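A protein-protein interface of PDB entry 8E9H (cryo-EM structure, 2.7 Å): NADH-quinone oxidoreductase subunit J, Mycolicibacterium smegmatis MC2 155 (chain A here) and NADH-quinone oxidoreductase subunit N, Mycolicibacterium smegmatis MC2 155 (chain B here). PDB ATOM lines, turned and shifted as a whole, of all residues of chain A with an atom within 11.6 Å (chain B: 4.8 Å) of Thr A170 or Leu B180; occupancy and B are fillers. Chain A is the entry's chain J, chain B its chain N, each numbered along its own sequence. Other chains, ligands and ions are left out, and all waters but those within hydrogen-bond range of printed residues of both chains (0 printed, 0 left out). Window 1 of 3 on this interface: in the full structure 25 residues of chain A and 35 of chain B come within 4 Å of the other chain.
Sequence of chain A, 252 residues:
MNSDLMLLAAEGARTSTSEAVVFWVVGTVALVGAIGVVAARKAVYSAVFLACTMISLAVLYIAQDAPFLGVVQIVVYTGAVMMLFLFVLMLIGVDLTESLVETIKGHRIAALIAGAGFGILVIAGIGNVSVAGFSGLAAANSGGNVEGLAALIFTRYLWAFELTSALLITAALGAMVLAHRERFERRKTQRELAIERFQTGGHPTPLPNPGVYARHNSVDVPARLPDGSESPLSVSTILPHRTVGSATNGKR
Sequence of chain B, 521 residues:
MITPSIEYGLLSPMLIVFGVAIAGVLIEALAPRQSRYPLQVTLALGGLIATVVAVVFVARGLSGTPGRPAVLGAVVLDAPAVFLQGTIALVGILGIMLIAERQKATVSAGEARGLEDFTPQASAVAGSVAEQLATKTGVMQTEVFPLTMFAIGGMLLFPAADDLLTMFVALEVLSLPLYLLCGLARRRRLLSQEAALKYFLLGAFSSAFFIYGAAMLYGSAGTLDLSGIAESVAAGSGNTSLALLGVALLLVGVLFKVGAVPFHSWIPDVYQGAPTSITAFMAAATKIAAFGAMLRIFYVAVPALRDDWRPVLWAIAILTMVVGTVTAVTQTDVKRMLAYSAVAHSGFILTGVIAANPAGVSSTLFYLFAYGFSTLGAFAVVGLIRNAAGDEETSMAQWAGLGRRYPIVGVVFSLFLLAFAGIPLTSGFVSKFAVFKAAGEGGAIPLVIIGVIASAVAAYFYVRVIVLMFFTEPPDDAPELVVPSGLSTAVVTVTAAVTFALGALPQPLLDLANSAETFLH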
ATOM      1  N   ALA A 160      -1.893  -5.652   6.108  1.00  0.00           N
ATOM      2  CA  ALA A 160      -1.265  -5.677   7.422  1.00  0.00           C
ATOM      3  C   ALA A 160       0.074  -6.395   7.368  1.00  0.00           C
ATOM      4  O   ALA A 160       1.035  -5.995   8.038  1.00  0.00           O
ATOM      5  CB  ALA A 160      -2.196  -6.349   8.429  1.00  0.00           C
ATOM      6  N   GLU A 162       2.175  -6.467   4.903  1.00  0.00           N
ATOM      7  CA  GLU A 162       3.156  -5.532   4.368  1.00  0.00           C
ATOM      8  C   GLU A 162       3.518  -4.470   5.395  1.00  0.00           C
ATOM      9  O   GLU A 162       4.693  -4.120   5.550  1.00  0.00           O
ATOM     10  CB  GLU A 162       2.615  -4.889   3.094  1.00  0.00           C
ATOM     11  CG  GLU A 162       2.376  -5.882   1.976  1.00  0.00           C
ATOM     12  CD  GLU A 162       3.661  -6.431   1.405  1.00  0.00           C
ATOM     13  OE1 GLU A 162       4.741  -6.041   1.889  1.00  0.00           O
ATOM     14  OE2 GLU A 162       3.591  -7.260   0.476  1.00  0.00           O
ATOM     15  N   LEU A 163       2.524  -3.948   6.115  1.00  0.00           N
ATOM     16  CA  LEU A 163       2.798  -2.917   7.109  1.00  0.00           C
ATOM     17  C   LEU A 163       3.669  -3.425   8.247  1.00  0.00           C
ATOM     18  O   LEU A 163       4.342  -2.625   8.911  1.00  0.00           O
ATOM     19  CB  LEU A 163       1.490  -2.374   7.668  1.00  0.00           C
ATOM     20  CG  LEU A 163       0.645  -1.624   6.647  1.00  0.00           C
ATOM     21  CD1 LEU A 163      -0.806  -1.647   7.063  1.00  0.00           C
ATOM     22  CD2 LEU A 163       1.140  -0.201   6.496  1.00  0.00           C
ATOM     23  N   THR A 164       3.654  -4.728   8.516  1.00  0.00           N
ATOM     24  CA  THR A 164       4.587  -5.253   9.505  1.00  0.00           C
ATOM     25  C   THR A 164       6.026  -4.975   9.099  1.00  0.00           C
ATOM     26  O   THR A 164       6.897  -4.817   9.960  1.00  0.00           O
ATOM     27  CB  THR A 164       4.372  -6.749   9.704  1.00  0.00           C
ATOM     28  OG1 THR A 164       4.350  -7.405   8.433  1.00  0.00           O
ATOM     29  CG2 THR A 164       3.067  -7.000  10.434  1.00  0.00           C
ATOM     30  N   SER A 165       6.295  -4.894   7.795  1.00  0.00           N
ATOM     31  CA  SER A 165       7.621  -4.483   7.350  1.00  0.00           C
ATOM     32  C   SER A 165       7.923  -3.055   7.773  1.00  0.00           C
ATOM     33  O   SER A 165       9.052  -2.748   8.165  1.00  0.00           O
ATOM     34  CB  SER A 165       7.733  -4.613   5.835  1.00  0.00           C
ATOM     35  OG  SER A 165       7.014  -3.579   5.190  1.00  0.00           O
ATOM     36  N   ALA A 166       6.933  -2.167   7.689  1.00  0.00           N
ATOM     37  CA  ALA A 166       7.127  -0.808   8.178  1.00  0.00           C
ATOM     38  C   ALA A 166       7.387  -0.804   9.676  1.00  0.00           C
ATOM     39  O   ALA A 166       8.218  -0.034  10.167  1.00  0.00           O
ATOM     40  CB  ALA A 166       5.910   0.050   7.844  1.00  0.00           C
ATOM     41  N   LEU A 167       6.678  -1.650  10.420  1.00  0.00           N
ATOM     42  CA  LEU A 167       6.948  -1.766  11.851  1.00  0.00           C
ATOM     43  C   LEU A 167       8.388  -2.191  12.098  1.00  0.00           C
ATOM     44  O   LEU A 167       9.077  -1.634  12.961  1.00  0.00           O
ATOM     45  CB  LEU A 167       5.983  -2.757  12.499  1.00  0.00           C
ATOM     46  CG  LEU A 167       4.516  -2.348  12.568  1.00  0.00           C
ATOM     47  CD1 LEU A 167       3.666  -3.502  13.055  1.00  0.00           C
ATOM     48  CD2 LEU A 167       4.365  -1.159  13.489  1.00  0.00           C
ATOM     49  N   LEU A 168       8.861  -3.185  11.348  1.00  0.00           N
ATOM     50  CA  LEU A 168      10.237  -3.644  11.503  1.00  0.00           C
ATOM     51  C   LEU A 168      11.224  -2.531  11.181  1.00  0.00           C
ATOM     52  O   LEU A 168      12.223  -2.344  11.885  1.00  0.00           O
ATOM     53  CB  LEU A 168      10.482  -4.857  10.607  1.00  0.00           C
ATOM     54  CG  LEU A 168      11.934  -5.149  10.226  1.00  0.00           C
ATOM     55  CD1 LEU A 168      12.744  -5.545  11.443  1.00  0.00           C
ATOM     56  CD2 LEU A 168      11.981  -6.241   9.183  1.00  0.00           C
ATOM     57  N   ILE A 169      10.969  -1.792  10.102  1.00  0.00           N
ATOM     58  CA  ILE A 169      11.877  -0.716   9.717  1.00  0.00           C
ATOM     59  C   ILE A 169      11.914   0.352  10.796  1.00  0.00           C
ATOM     60  O   ILE A 169      12.976   0.886  11.125  1.00  0.00           O
ATOM     61  CB  ILE A 169      11.469  -0.119   8.360  1.00  0.00           C
ATOM     62  CG1 ILE A 169      12.034  -0.960   7.223  1.00  0.00           C
ATOM     63  CG2 ILE A 169      11.986   1.303   8.247  1.00  0.00           C
ATOM     64  CD1 ILE A 169      11.471  -0.622   5.875  1.00  0.00           C
ATOM     65  N   THR A 170      10.751   0.709  11.336  1.00  0.00           N
ATOM     66  CA  THR A 170      10.718   1.714  12.390  1.00  0.00           C
ATOM     67  C   THR A 170      11.467   1.230  13.620  1.00  0.00           C
ATOM     68  O   THR A 170      12.182   2.003  14.261  1.00  0.00           O
ATOM     69  CB  THR A 170       9.277   2.064  12.750  1.00  0.00           C
ATOM     70  OG1 THR A 170       8.569   0.874  13.114  1.00  0.00           O
ATOM     71  CG2 THR A 170       8.584   2.729  11.577  1.00  0.00           C
ATOM     72  N   ALA A 171      11.317  -0.047  13.967  1.00  0.00           N
ATOM     73  CA  ALA A 171      12.055  -0.584  15.103  1.00  0.00           C
ATOM     74  C   ALA A 171      13.557  -0.491  14.867  1.00  0.00           C
ATOM     75  O   ALA A 171      14.314  -0.076  15.751  1.00  0.00           O
ATOM     76  CB  ALA A 171      11.641  -2.031  15.359  1.00  0.00           C
ATOM     77  N   ALA A 172      14.004  -0.872  13.670  1.00  0.00           N
ATOM     78  CA  ALA A 172      15.430  -0.820  13.368  1.00  0.00           C
ATOM     79  C   ALA A 172      15.942   0.613  13.398  1.00  0.00           C
ATOM     80  O   ALA A 172      17.016   0.893  13.943  1.00  0.00           O
ATOM     81  CB  ALA A 172      15.697  -1.456  12.005  1.00  0.00           C
ATOM     82  N   LEU A 173      15.180   1.539  12.817  1.00  0.00           N
ATOM     83  CA  LEU A 173      15.581   2.939  12.817  1.00  0.00           C
ATOM     84  C   LEU A 173      15.660   3.481  14.233  1.00  0.00           C
ATOM     85  O   LEU A 173      16.586   4.223  14.568  1.00  0.00           O
ATOM     86  CB  LEU A 173      14.603   3.767  11.992  1.00  0.00           C
ATOM     87  CG  LEU A 173      14.741   3.667  10.479  1.00  0.00           C
ATOM     88  CD1 LEU A 173      13.473   4.158   9.816  1.00  0.00           C
ATOM     89  CD2 LEU A 173      15.930   4.474  10.012  1.00  0.00           C
ATOM     90  N   GLY A 174      14.686   3.140  15.073  1.00  0.00           N
ATOM     91  CA  GLY A 174      14.730   3.593  16.450  1.00  0.00           C
ATOM     92  C   GLY A 174      15.934   3.049  17.187  1.00  0.00           C
ATOM     93  O   GLY A 174      16.626   3.777  17.900  1.00  0.00           O
ATOM     94  N   ALA A 175      16.208   1.757  17.014  1.00  0.00           N
ATOM     95  CA  ALA A 175      17.362   1.164  17.675  1.00  0.00           C
ATOM     96  C   ALA A 175      18.645   1.852  17.234  1.00  0.00           C
ATOM     97  O   ALA A 175      19.517   2.152  18.055  1.00  0.00           O
ATOM     98  CB  ALA A 175      17.422  -0.333  17.377  1.00  0.00           C
ATOM     99  N   MET A 176      18.773   2.117  15.936  1.00  0.00           N
ATOM    100  CA  MET A 176      19.984   2.762  15.442  1.00  0.00           C
ATOM    101  C   MET A 176      20.092   4.200  15.933  1.00  0.00           C
ATOM    102  O   MET A 176      21.175   4.649  16.321  1.00  0.00           O
ATOM    103  CB  MET A 176      20.012   2.717  13.919  1.00  0.00           C
ATOM    104  CG  MET A 176      20.358   1.357  13.361  1.00  0.00           C
ATOM    105  SD  MET A 176      22.051   0.889  13.742  1.00  0.00           S
ATOM    106  CE  MET A 176      22.934   1.721  12.430  1.00  0.00           C
ATOM    107  N   VAL A 177      18.989   4.941  15.919  1.00  0.00           N
ATOM    108  CA  VAL A 177      19.047   6.356  16.260  1.00  0.00           C
ATOM    109  C   VAL A 177      19.305   6.539  17.748  1.00  0.00           C
ATOM    110  O   VAL A 177      20.145   7.349  18.152  1.00  0.00           O
ATOM    111  CB  VAL A 177      17.752   7.059  15.819  1.00  0.00           C
ATOM    112  CG1 VAL A 177      17.652   8.432  16.448  1.00  0.00           C
ATOM    113  CG2 VAL A 177      17.700   7.159  14.308  1.00  0.00           C
ATOM    114  N   LEU A 178      18.598   5.788  18.586  1.00  0.00           N
ATOM    115  CA  LEU A 178      18.653   6.017  20.023  1.00  0.00           C
ATOM    116  C   LEU A 178      19.758   5.237  20.715  1.00  0.00           C
ATOM    117  O   LEU A 178      20.275   5.697  21.739  1.00  0.00           O
ATOM    118  CB  LEU A 178      17.315   5.650  20.665  1.00  0.00           C
ATOM    119  CG  LEU A 178      16.134   6.557  20.330  1.00  0.00           C
ATOM    120  CD1 LEU A 178      14.865   6.016  20.952  1.00  0.00           C
ATOM    121  CD2 LEU A 178      16.394   7.969  20.805  1.00  0.00           C
ATOM    122  N   ALA A 179      20.133   4.078  20.194  1.00  0.00           N
ATOM    123  CA  ALA A 179      21.047   3.191  20.893  1.00  0.00           C
ATOM    124  C   ALA A 179      22.404   3.046  20.228  1.00  0.00           C
ATOM    125  O   ALA A 179      23.387   2.796  20.926  1.00  0.00           O
ATOM    126  CB  ALA A 179      20.421   1.797  21.037  1.00  0.00           C
ATOM    127  N   HIS A 180      22.491   3.196  18.912  1.00  0.00           N
ATOM    128  CA  HIS A 180      23.765   3.018  18.229  1.00  0.00           C
ATOM    129  C   HIS A 180      24.652   4.237  18.436  1.00  0.00           C
ATOM    130  O   HIS A 180      24.452   5.275  17.798  1.00  0.00           O
ATOM    131  CB  HIS A 180      23.545   2.780  16.741  1.00  0.00           C
ATOM    132  CG  HIS A 180      24.802   2.464  15.999  1.00  0.00           C
ATOM    133  ND1 HIS A 180      25.237   3.209  14.925  1.00  0.00           N
ATOM    134  CD2 HIS A 180      25.728   1.496  16.187  1.00  0.00           C
ATOM    135  CE1 HIS A 180      26.373   2.706  14.476  1.00  0.00           C
ATOM    136  NE2 HIS A 180      26.693   1.666  15.225  1.00  0.00           N
ATOM    137  N   LEU B 147      11.366   8.106   9.624  1.00  0.00           N
ATOM    138  CA  LEU B 147      10.453   7.825  10.725  1.00  0.00           C
ATOM    139  C   LEU B 147       9.192   8.663  10.603  1.00  0.00           C
ATOM    140  O   LEU B 147       8.076   8.130  10.605  1.00  0.00           O
ATOM    141  CB  LEU B 147      11.144   8.100  12.058  1.00  0.00           C
ATOM    142  CG  LEU B 147      12.204   7.097  12.499  1.00  0.00           C
ATOM    143  CD1 LEU B 147      12.938   7.618  13.718  1.00  0.00           C
ATOM    144  CD2 LEU B 147      11.577   5.752  12.790  1.00  0.00           C
ATOM    145  N   PHE B 150       6.949   7.358   8.010  1.00  0.00           N
ATOM    146  CA  PHE B 150       6.251   6.176   8.494  1.00  0.00           C
ATOM    147  C   PHE B 150       5.082   6.568   9.381  1.00  0.00           C
ATOM    148  O   PHE B 150       3.959   6.096   9.173  1.00  0.00           O
ATOM    149  CB  PHE B 150       7.212   5.259   9.240  1.00  0.00           C
ATOM    150  CG  PHE B 150       8.013   4.382   8.339  1.00  0.00           C
ATOM    151  CD1 PHE B 150       7.398   3.393   7.598  1.00  0.00           C
ATOM    152  CD2 PHE B 150       9.375   4.551   8.219  1.00  0.00           C
ATOM    153  CE1 PHE B 150       8.126   2.586   6.761  1.00  0.00           C
ATOM    154  CE2 PHE B 150      10.108   3.746   7.383  1.00  0.00           C
ATOM    155  CZ  PHE B 150       9.483   2.762   6.653  1.00  0.00           C
ATOM    156  N   LEU B 176       4.891   3.903  17.017  1.00  0.00           N
ATOM    157  CA  LEU B 176       6.314   3.650  17.240  1.00  0.00           C
ATOM    158  C   LEU B 176       7.187   4.795  16.750  1.00  0.00           C
ATOM    159  O   LEU B 176       8.037   5.274  17.526  1.00  0.00           O
ATOM    160  CB  LEU B 176       6.715   2.323  16.590  1.00  0.00           C
ATOM    161  CG  LEU B 176       6.029   1.069  17.129  1.00  0.00           C
ATOM    162  CD1 LEU B 176       6.588  -0.165  16.448  1.00  0.00           C
ATOM    163  CD2 LEU B 176       6.176   0.958  18.632  1.00  0.00           C
ATOM    164  N   PRO B 177       7.042   5.288  15.520  1.00  0.00           N
ATOM    165  CA  PRO B 177       7.878   6.418  15.095  1.00  0.00           C
ATOM    166  C   PRO B 177       7.730   7.620  15.998  1.00  0.00           C
ATOM    167  O   PRO B 177       8.707   8.333  16.239  1.00  0.00           O
ATOM    168  CB  PRO B 177       7.374   6.704  13.678  1.00  0.00           C
ATOM    169  CG  PRO B 177       6.795   5.431  13.226  1.00  0.00           C
ATOM    170  CD  PRO B 177       6.151   4.852  14.438  1.00  0.00           C
ATOM    171  N   LEU B 178       6.530   7.862  16.517  1.00  0.00           N
ATOM    172  CA  LEU B 178       6.343   8.990  17.418  1.00  0.00           C
ATOM    173  C   LEU B 178       7.013   8.735  18.760  1.00  0.00           C
ATOM    174  O   LEU B 178       7.628   9.642  19.334  1.00  0.00           O
ATOM    175  CB  LEU B 178       4.854   9.264  17.594  1.00  0.00           C
ATOM    176  CG  LEU B 178       4.152   9.690  16.305  1.00  0.00           C
ATOM    177  CD1 LEU B 178       2.657   9.666  16.506  1.00  0.00           C
ATOM    178  CD2 LEU B 178       4.604  11.064  15.836  1.00  0.00           C
ATOM    179  N   TYR B 179       6.911   7.509  19.279  1.00  0.00           N
ATOM    180  CA  TYR B 179       7.665   7.172  20.479  1.00  0.00           C
ATOM    181  C   TYR B 179       9.128   7.528  20.294  1.00  0.00           C
ATOM    182  O   TYR B 179       9.738   8.166  21.158  1.00  0.00           O
ATOM    183  CB  TYR B 179       7.550   5.685  20.804  1.00  0.00           C
ATOM    184  CG  TYR B 179       6.155   5.175  21.056  1.00  0.00           C
ATOM    185  CD1 TYR B 179       5.163   6.003  21.541  1.00  0.00           C
ATOM    186  CD2 TYR B 179       5.843   3.849  20.824  1.00  0.00           C
ATOM    187  CE1 TYR B 179       3.893   5.526  21.769  1.00  0.00           C
ATOM    188  CE2 TYR B 179       4.585   3.365  21.050  1.00  0.00           C
ATOM    189  CZ  TYR B 179       3.613   4.203  21.526  1.00  0.00           C
ATOM    190  OH  TYR B 179       2.354   3.704  21.745  1.00  0.00           O
ATOM    191  N   LEU B 180       9.705   7.127  19.163  1.00  0.00           N
ATOM    192  CA  LEU B 180      11.118   7.399  18.926  1.00  0.00           C
ATOM    193  C   LEU B 180      11.379   8.893  18.799  1.00  0.00           C
ATOM    194  O   LEU B 180      12.325   9.421  19.391  1.00  0.00           O
ATOM    195  CB  LEU B 180      11.583   6.665  17.673  1.00  0.00           C
ATOM    196  CG  LEU B 180      11.466   5.147  17.772  1.00  0.00           C
ATOM    197  CD1 LEU B 180      11.570   4.516  16.401  1.00  0.00           C
ATOM    198  CD2 LEU B 180      12.527   4.608  18.705  1.00  0.00           C
ATOM    199  N   LEU B 181      10.541   9.595  18.038  1.00  0.00           N
ATOM    200  CA  LEU B 181      10.794  11.002  17.761  1.00  0.00           C
ATOM    201  C   LEU B 181      10.692  11.851  19.016  1.00  0.00           C
ATOM    202  O   LEU B 181      11.352  12.889  19.116  1.00  0.00           O
ATOM    203  CB  LEU B 181       9.816  11.509  16.706  1.00  0.00           C
ATOM    204  CG  LEU B 181      10.013  10.929  15.309  1.00  0.00           C
ATOM    205  CD1 LEU B 181       8.749  11.082  14.491  1.00  0.00           C
ATOM    206  CD2 LEU B 181      11.180  11.599  14.623  1.00  0.00           C
ATOM    207  N   CYS B 182       9.872  11.439  19.982  1.00  0.00           N
ATOM    208  CA  CYS B 182       9.730  12.234  21.194  1.00  0.00           C
ATOM    209  C   CYS B 182      11.045  12.406  21.940  1.00  0.00           C
ATOM    210  O   CYS B 182      11.186  13.365  22.703  1.00  0.00           O
ATOM    211  CB  CYS B 182       8.702  11.601  22.125  1.00  0.00           C
ATOM    212  SG  CYS B 182       7.002  11.888  21.630  1.00  0.00           S
ATOM    213  N   GLY B 183      12.006  11.512  21.741  1.00  0.00           N
ATOM    214  CA  GLY B 183      13.237  11.546  22.497  1.00  0.00           C
ATOM    215  C   GLY B 183      14.433  12.132  21.789  1.00  0.00           C
ATOM    216  O   GLY B 183      15.563  11.908  22.231  1.00  0.00           O
ATOM    217  N   LEU B 184      14.235  12.879  20.705  1.00  0.00           N
ATOM    218  CA  LEU B 184      15.339  13.374  19.896  1.00  0.00           C
ATOM    219  C   LEU B 184      15.577  14.870  20.064  1.00  0.00           C
ATOM    220  O   LEU B 184      16.364  15.446  19.310  1.00  0.00           O
ATOM    221  CB  LEU B 184      15.089  13.055  18.424  1.00  0.00           C
ATOM    222  CG  LEU B 184      14.685  11.616  18.117  1.00  0.00           C
ATOM    223  CD1 LEU B 184      14.530  11.422  16.625  1.00  0.00           C
ATOM    224  CD2 LEU B 184      15.700  10.640  18.675  1.00  0.00           C
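O of Ala A166 is in hydrogen-bond range of OG1 of Thr A170 (3.1 Å).
The side-chain hydroxyl of Thr A170 is in hydrogen-bond range of the backbone carbonyl oxygen of Leu A167, at 2.6 Å.
Ala A166 touches Phe B150.
CD2 of Leu A167 touches CD1 of Leu B176 (3.8 Å).
Ile A169 touches Phe B150.
CG2 of Thr A170 touches CG of Phe B150, 3.7 Å away.
Pro B177 touches Thr A170 (CG to CG2, 3.6 Å).
O of Thr A170 touches CD1 of Leu B180, 3.4 Å away.
CB of Leu A173 touches CD2 of Leu B147, at 3.7 Å.
Gly A174 touches Leu B180.
Leu B184 touches Val A177.
Leu B184 touches Leu A178.
Of the printed residues of chain B, Thr A170 touches Phe B150 (3.7 Å), Pro B177 (3.6 Å) and Leu B180 (3.4 Å).
Printed residues of chain A within 4 Å of Leu B147: Leu A173 (3.7 Å).
Pro B177 touches just one residue of chain A: Thr A170.
No residue of chain A comes within 4 Å of Cys B182.
No residue of chain A comes within 4 Å of Gly B183.
Leu B184 touches just these residues of chain A: Val A177 and Leu A178.
Of the printed residues of chain B, Leu A173 touches Leu B147.
Of the printed residues of chain B, Leu A167 touches Leu B176 (3.8 Å).
Of the printed residues of chain B, Leu A178 touches Leu B180 and Leu B184.
Of the printed residues of chain B, Ile A169 touches Phe B150.
Of the printed residues of chain B, Gly A174 touches Leu B180 (3.3 Å).
Ala A175 touches none of the printed residues of chain B.
Glu A162 touches none of the printed residues of chain B.
Of the 11 printed residues of chain B, 6 touch a printed residue of chain A.
Among the printed residues, 11 pairs touch across the chains.
Among the printed residues, no Asp or Glu carboxylate lies within 4 Å of a Lys or Arg side-chain nitrogen of the other chain.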
